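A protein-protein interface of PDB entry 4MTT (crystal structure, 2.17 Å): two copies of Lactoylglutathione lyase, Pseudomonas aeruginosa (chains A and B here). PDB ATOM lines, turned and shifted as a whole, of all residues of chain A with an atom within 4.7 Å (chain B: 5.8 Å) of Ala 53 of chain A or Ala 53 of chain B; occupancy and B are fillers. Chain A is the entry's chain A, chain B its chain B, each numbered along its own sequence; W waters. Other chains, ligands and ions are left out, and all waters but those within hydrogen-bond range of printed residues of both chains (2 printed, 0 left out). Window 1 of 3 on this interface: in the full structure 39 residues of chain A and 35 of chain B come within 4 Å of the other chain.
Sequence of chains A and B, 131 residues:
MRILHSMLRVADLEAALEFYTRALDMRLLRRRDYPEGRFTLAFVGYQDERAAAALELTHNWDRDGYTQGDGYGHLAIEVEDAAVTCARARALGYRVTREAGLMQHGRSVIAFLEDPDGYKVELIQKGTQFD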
ATOM      1  N   ILE A   3     -32.533  -7.794 -30.364  1.00  0.00           N
ATOM      2  CA  ILE A   3     -31.457  -8.409 -31.130  1.00  0.00           C
ATOM      3  C   ILE A   3     -31.996  -9.766 -31.635  1.00  0.00           C
ATOM      4  O   ILE A   3     -32.510 -10.543 -30.835  1.00  0.00           O
ATOM      5  CB  ILE A   3     -30.144  -8.500 -30.307  1.00  0.00           C
ATOM      6  CG1 ILE A   3     -29.578  -7.087 -30.062  1.00  0.00           C
ATOM      7  CG2 ILE A   3     -29.106  -9.381 -31.040  1.00  0.00           C
ATOM      8  CD1 ILE A   3     -28.542  -6.912 -28.903  1.00  0.00           C
ATOM      9  N   LEU A   4     -31.978  -9.995 -32.958  1.00  0.00           N
ATOM     10  CA  LEU A   4     -32.526 -11.223 -33.545  1.00  0.00           C
ATOM     11  C   LEU A   4     -31.535 -12.369 -33.657  1.00  0.00           C
ATOM     12  O   LEU A   4     -31.842 -13.487 -33.251  1.00  0.00           O
ATOM     13  CB  LEU A   4     -33.214 -10.969 -34.913  1.00  0.00           C
ATOM     14  CG  LEU A   4     -34.483 -10.109 -34.859  1.00  0.00           C
ATOM     15  CD1 LEU A   4     -34.899  -9.664 -36.245  1.00  0.00           C
ATOM     16  CD2 LEU A   4     -35.628 -10.811 -34.111  1.00  0.00           C
ATOM     17  N   HIS A   5     -30.368 -12.105 -34.228  1.00  0.00           N
ATOM     18  CA  HIS A   5     -29.370 -13.142 -34.428  1.00  0.00           C
ATOM     19  C   HIS A   5     -28.060 -12.541 -34.793  1.00  0.00           C
ATOM     20  O   HIS A   5     -28.005 -11.389 -35.177  1.00  0.00           O
ATOM     21  CB  HIS A   5     -29.796 -14.169 -35.531  1.00  0.00           C
ATOM     22  CG  HIS A   5     -30.067 -13.586 -36.885  1.00  0.00           C
ATOM     23  ND1 HIS A   5     -31.367 -13.335 -37.320  1.00  0.00           N
ATOM     24  CD2 HIS A   5     -29.206 -13.274 -37.880  1.00  0.00           C
ATOM     25  CE1 HIS A   5     -31.252 -12.879 -38.557  1.00  0.00           C
ATOM     26  NE2 HIS A   5     -29.968 -12.802 -38.930  1.00  0.00           N
ATOM     27  N   ALA A  52     -35.997 -15.243 -28.353  1.00  0.00           N
ATOM     28  CA  ALA A  52     -34.600 -14.949 -28.070  1.00  0.00           C
ATOM     29  C   ALA A  52     -33.740 -14.851 -29.319  1.00  0.00           C
ATOM     30  O   ALA A  52     -34.111 -15.353 -30.384  1.00  0.00           O
ATOM     31  CB  ALA A  52     -34.031 -16.064 -27.165  1.00  0.00           C
ATOM     32  N   ALA A  53     -32.538 -14.276 -29.142  1.00  0.00           N
ATOM     33  CA  ALA A  53     -31.536 -14.149 -30.191  1.00  0.00           C
ATOM     34  C   ALA A  53     -30.988 -15.539 -30.505  1.00  0.00           C
ATOM     35  O   ALA A  53     -30.827 -16.371 -29.608  1.00  0.00           O
ATOM     36  CB  ALA A  53     -30.408 -13.206 -29.743  1.00  0.00           C
ATOM     37  N   ALA A  54     -30.736 -15.805 -31.781  1.00  0.00           N
ATOM     38  CA  ALA A  54     -30.214 -17.103 -32.205  1.00  0.00           C
ATOM     39  C   ALA A  54     -28.885 -16.927 -32.941  1.00  0.00           C
ATOM     40  O   ALA A  54     -28.435 -15.807 -33.179  1.00  0.00           O
ATOM     41  CB  ALA A  54     -31.227 -17.789 -33.119  1.00  0.00           C
ATOM     42  N   LEU A  55     -28.267 -18.038 -33.296  1.00  0.00           N
ATOM     43  CA  LEU A  55     -27.064 -18.065 -34.085  1.00  0.00           C
ATOM     44  C   LEU A  55     -27.430 -18.508 -35.534  1.00  0.00           C
ATOM     45  O   LEU A  55     -27.971 -19.595 -35.738  1.00  0.00           O
ATOM     46  CB  LEU A  55     -26.033 -19.002 -33.447  1.00  0.00           C
ATOM     47  CG  LEU A  55     -24.726 -19.223 -34.260  1.00  0.00           C
ATOM     48  CD1 LEU A  55     -23.970 -17.906 -34.452  1.00  0.00           C
ATOM     49  CD2 LEU A  55     -23.856 -20.225 -33.574  1.00  0.00           C
ATOM     50  N   ARG B   2     -28.306 -20.364 -22.250  1.00  0.00           N
ATOM     51  CA  ARG B   2     -28.788 -19.248 -23.062  1.00  0.00           C
ATOM     52  C   ARG B   2     -27.645 -18.483 -23.703  1.00  0.00           C
ATOM     53  O   ARG B   2     -26.509 -18.545 -23.210  1.00  0.00           O
ATOM     54  CB  ARG B   2     -29.784 -18.336 -22.313  1.00  0.00           C
ATOM     55  CG  ARG B   2     -29.156 -17.380 -21.342  1.00  0.00           C
ATOM     56  CD  ARG B   2     -30.199 -16.648 -20.535  1.00  0.00           C
ATOM     57  NE  ARG B   2     -29.530 -15.875 -19.489  1.00  0.00           N
ATOM     58  CZ  ARG B   2     -29.288 -14.567 -19.548  1.00  0.00           C
ATOM     59  NH1 ARG B   2     -29.708 -13.850 -20.585  1.00  0.00           N
ATOM     60  NH2 ARG B   2     -28.646 -13.965 -18.562  1.00  0.00           N
ATOM     61  N   ILE B   3     -27.930 -17.810 -24.827  1.00  0.00           N
ATOM     62  CA  ILE B   3     -26.938 -16.977 -25.519  1.00  0.00           C
ATOM     63  C   ILE B   3     -26.854 -15.683 -24.702  1.00  0.00           C
ATOM     64  O   ILE B   3     -27.874 -15.051 -24.462  1.00  0.00           O
ATOM     65  CB  ILE B   3     -27.296 -16.709 -27.017  1.00  0.00           C
ATOM     66  CG1 ILE B   3     -27.269 -18.038 -27.837  1.00  0.00           C
ATOM     67  CG2 ILE B   3     -26.325 -15.652 -27.624  1.00  0.00           C
ATOM     68  CD1 ILE B   3     -27.851 -18.016 -29.325  1.00  0.00           C
ATOM     69  N   LEU B   4     -25.658 -15.318 -24.261  1.00  0.00           N
ATOM     70  CA  LEU B   4     -25.453 -14.103 -23.454  1.00  0.00           C
ATOM     71  C   LEU B   4     -25.151 -12.885 -24.283  1.00  0.00           C
ATOM     72  O   LEU B   4     -25.728 -11.832 -24.045  1.00  0.00           O
ATOM     73  CB  LEU B   4     -24.332 -14.313 -22.439  1.00  0.00           C
ATOM     74  CG  LEU B   4     -24.629 -15.293 -21.298  1.00  0.00           C
ATOM     75  CD1 LEU B   4     -23.319 -15.628 -20.537  1.00  0.00           C
ATOM     76  CD2 LEU B   4     -25.655 -14.673 -20.294  1.00  0.00           C
ATOM     77  N   HIS B   5     -24.217 -13.006 -25.226  1.00  0.00           N
ATOM     78  CA  HIS B   5     -23.844 -11.885 -26.080  1.00  0.00           C
ATOM     79  C   HIS B   5     -23.028 -12.343 -27.296  1.00  0.00           C
ATOM     80  O   HIS B   5     -22.539 -13.466 -27.342  1.00  0.00           O
ATOM     81  CB  HIS B   5     -23.042 -10.794 -25.270  1.00  0.00           C
ATOM     82  CG  HIS B   5     -21.783 -11.268 -24.591  1.00  0.00           C
ATOM     83  ND1 HIS B   5     -21.774 -11.628 -23.242  1.00  0.00           N
ATOM     84  CD2 HIS B   5     -20.515 -11.340 -25.061  1.00  0.00           C
ATOM     85  CE1 HIS B   5     -20.526 -11.962 -22.959  1.00  0.00           C
ATOM     86  NE2 HIS B   5     -19.730 -11.815 -24.019  1.00  0.00           N
ATOM     87  N   VAL B  44     -24.251  -3.121 -24.970  1.00  0.00           N
ATOM     88  CA  VAL B  44     -25.390  -2.371 -25.508  1.00  0.00           C
ATOM     89  C   VAL B  44     -26.529  -3.315 -25.838  1.00  0.00           C
ATOM     90  O   VAL B  44     -26.283  -4.462 -26.189  1.00  0.00           O
ATOM     91  CB  VAL B  44     -25.023  -1.435 -26.697  1.00  0.00           C
ATOM     92  CG1 VAL B  44     -24.163  -0.266 -26.232  1.00  0.00           C
ATOM     93  CG2 VAL B  44     -24.350  -2.195 -27.834  1.00  0.00           C
ATOM     94  N   GLY B  45     -27.760  -2.833 -25.749  1.00  0.00           N
ATOM     95  CA  GLY B  45     -28.902  -3.682 -26.074  1.00  0.00           C
ATOM     96  C   GLY B  45     -30.238  -3.046 -25.815  1.00  0.00           C
ATOM     97  O   GLY B  45     -30.325  -1.842 -25.588  1.00  0.00           O
ATOM     98  N   ASP B  48     -32.633  -6.017 -20.355  1.00  0.00           N
ATOM     99  CA  ASP B  48     -31.713  -6.372 -19.249  1.00  0.00           C
ATOM    100  C   ASP B  48     -30.946  -7.614 -19.698  1.00  0.00           C
ATOM    101  O   ASP B  48     -31.526  -8.493 -20.349  1.00  0.00           O
ATOM    102  CB  ASP B  48     -32.463  -6.690 -17.919  1.00  0.00           C
ATOM    103  CG  ASP B  48     -31.684  -7.210 -16.671  1.00  0.00           C
ATOM    104  OD1 ASP B  48     -30.414  -7.275 -16.709  1.00  0.00           O
ATOM    105  OD2 ASP B  48     -32.337  -7.503 -15.649  1.00  0.00           O
ATOM    106  N   GLU B  49     -29.633  -7.650 -19.411  1.00  0.00           N
ATOM    107  CA  GLU B  49     -28.732  -8.752 -19.757  1.00  0.00           C
ATOM    108  C   GLU B  49     -29.210 -10.104 -19.225  1.00  0.00           C
ATOM    109  O   GLU B  49     -28.967 -11.129 -19.862  1.00  0.00           O
ATOM    110  CB  GLU B  49     -27.323  -8.452 -19.237  1.00  0.00           C
ATOM    111  CG  GLU B  49     -26.615  -7.404 -20.071  1.00  0.00           C
ATOM    112  CD  GLU B  49     -25.171  -7.190 -19.676  1.00  0.00           C
ATOM    113  OE1 GLU B  49     -24.279  -7.777 -20.332  1.00  0.00           O
ATOM    114  OE2 GLU B  49     -24.934  -6.439 -18.704  1.00  0.00           O
ATOM    115  N   ALA B  51     -32.301 -11.025 -19.043  1.00  0.00           N
ATOM    116  CA  ALA B  51     -33.465 -11.402 -19.847  1.00  0.00           C
ATOM    117  C   ALA B  51     -33.185 -11.664 -21.338  1.00  0.00           C
ATOM    118  O   ALA B  51     -34.002 -12.307 -22.014  1.00  0.00           O
ATOM    119  CB  ALA B  51     -34.531 -10.314 -19.724  1.00  0.00           C
ATOM    120  N   ALA B  52     -32.102 -11.072 -21.885  1.00  0.00           N
ATOM    121  CA  ALA B  52     -31.825 -11.176 -23.317  1.00  0.00           C
ATOM    122  C   ALA B  52     -30.352 -11.035 -23.633  1.00  0.00           C
ATOM    123  O   ALA B  52     -29.585 -10.500 -22.822  1.00  0.00           O
ATOM    124  CB  ALA B  52     -32.641 -10.130 -24.090  1.00  0.00           C
ATOM    125  N   ALA B  53     -29.958 -11.539 -24.815  1.00  0.00           N
ATOM    126  CA  ALA B  53     -28.586 -11.473 -25.291  1.00  0.00           C
ATOM    127  C   ALA B  53     -28.297 -10.026 -25.703  1.00  0.00           C
ATOM    128  O   ALA B  53     -29.161  -9.340 -26.246  1.00  0.00           O
ATOM    129  CB  ALA B  53     -28.370 -12.423 -26.480  1.00  0.00           C
ATOM    130  N   ALA B  54     -27.090  -9.575 -25.432  1.00  0.00           N
ATOM    131  CA  ALA B  54     -26.683  -8.210 -25.757  1.00  0.00           C
ATOM    132  C   ALA B  54     -25.575  -8.210 -26.781  1.00  0.00           C
ATOM    133  O   ALA B  54     -25.164  -9.263 -27.254  1.00  0.00           O
ATOM    134  CB  ALA B  54     -26.197  -7.504 -24.490  1.00  0.00           C
ATOM    135  N   LEU B  55     -25.038  -7.021 -27.057  1.00  0.00           N
ATOM    136  CA  LEU B  55     -23.880  -6.825 -27.905  1.00  0.00           C
ATOM    137  C   LEU B  55     -22.719  -6.292 -27.023  1.00  0.00           C
ATOM    138  O   LEU B  55     -22.821  -5.219 -26.422  1.00  0.00           O
ATOM    139  CB  LEU B  55     -24.209  -5.834 -29.029  1.00  0.00           C
ATOM    140  CG  LEU B  55     -23.024  -5.441 -29.919  1.00  0.00           C
ATOM    141  CD1 LEU B  55     -22.415  -6.681 -30.629  1.00  0.00           C
ATOM    142  CD2 LEU B  55     -23.439  -4.341 -30.911  1.00  0.00           C
HETATM  143  O   HOH W   1     -32.014 -13.115 -26.434  1.00  0.00           O
HETATM  144  O   HOH W   2     -31.510 -10.300 -27.639  1.00  0.00           O
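Among the printed residues, merely in contact across the chains: Ala 53 of chain A with Ile 3 of chain B, Ile 3 of chain A with Ala 53 of chain B, Ala 54 of chain A with Ile 3 of chain B, Ile 3 of chain A with Ala 54 of chain B, Ala 53 of chain A with Ala 53 of chain B, Ile 3 of chain A with Leu 55 of chain B and Leu 55 of chain A with Ile 3 of chain B.
O of Leu 4 of chain A sits at hydrogen-bond distance from N of Ala 54 of chain A, at 3.0 Å.
The backbone NH (N) of Ala 54 of chain B sits at hydrogen-bond distance from the backbone carbonyl oxygen (O) of Leu 4 of chain B, at 3.0 Å.
The backbone NH (N) of Val 44 of chain B lies within hydrogen-bond range of the backbone carbonyl oxygen (O) of Leu 55 of chain B (2.9 Å).
Water W2 bridges O of Ala 53 of chain B and O of Ile 3 of chain A.
Water W1 lies within hydrogen-bond range of the backbone NH (N) of Ala 53 of chain A and the backbone NH (N) of Ala 53 of chain B.
Printed residues of chain A that touch a printed residue of chain B: Ile 3, Ala 53, Ala 54 and Leu 55.
Of chain B, only Ile 3 and Ala 53 come within 4 Å of Ala 53 of chain A.
Ala 53 of chain B touches two residues of chain A.
Printed residues of chain B within 4 Å of Ile 3 of chain A: Ala 53 (3.7 Å), Ala 54 (3.9 Å) and Leu 55 (3.96 Å).
Of the printed residues of chain A, Ala 54 of chain B touches Ile 3.
Of the printed residues of chain B, Ala 54 of chain A touches Ile 3.
Printed residues of chain A within 4 Å of Ile 3 of chain B: Ala 53 (3.4 Å), Ala 54 (3.8 Å) and Leu 55 (3.99 Å).
Asp 48 of chain B touches none of the printed residues of chain A.
His 5 of chain B touches none of the printed residues of chain A.
The nearest printed residue of chain B that does not touch Ala 53 of chain A is Ala 52 of chain B (6.5 Å).
Ile 3 of chain A touches Ala 53 of chain B, and with the chains exchanged Ala 53 of chain A touches Ile 3 of chain B.
Ile 3 of chain A touches Ala 54 of chain B, and with the chains exchanged Ala 54 of chain A touches Ile 3 of chain B.
Ile 3 of chain A touches Leu 55 of chain B, and with the chains exchanged Leu 55 of chain A touches Ile 3 of chain B.
Ala 53 of chain B touches its own counterpart, Ala 53 of chain A.
Positions printed for both chains: 3, 4, 5, 52, 53, 54 and 55.
Of the 7 pairs that touch across the chains among the printed residues, 7 have their exchanged pair printed and touching as well.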
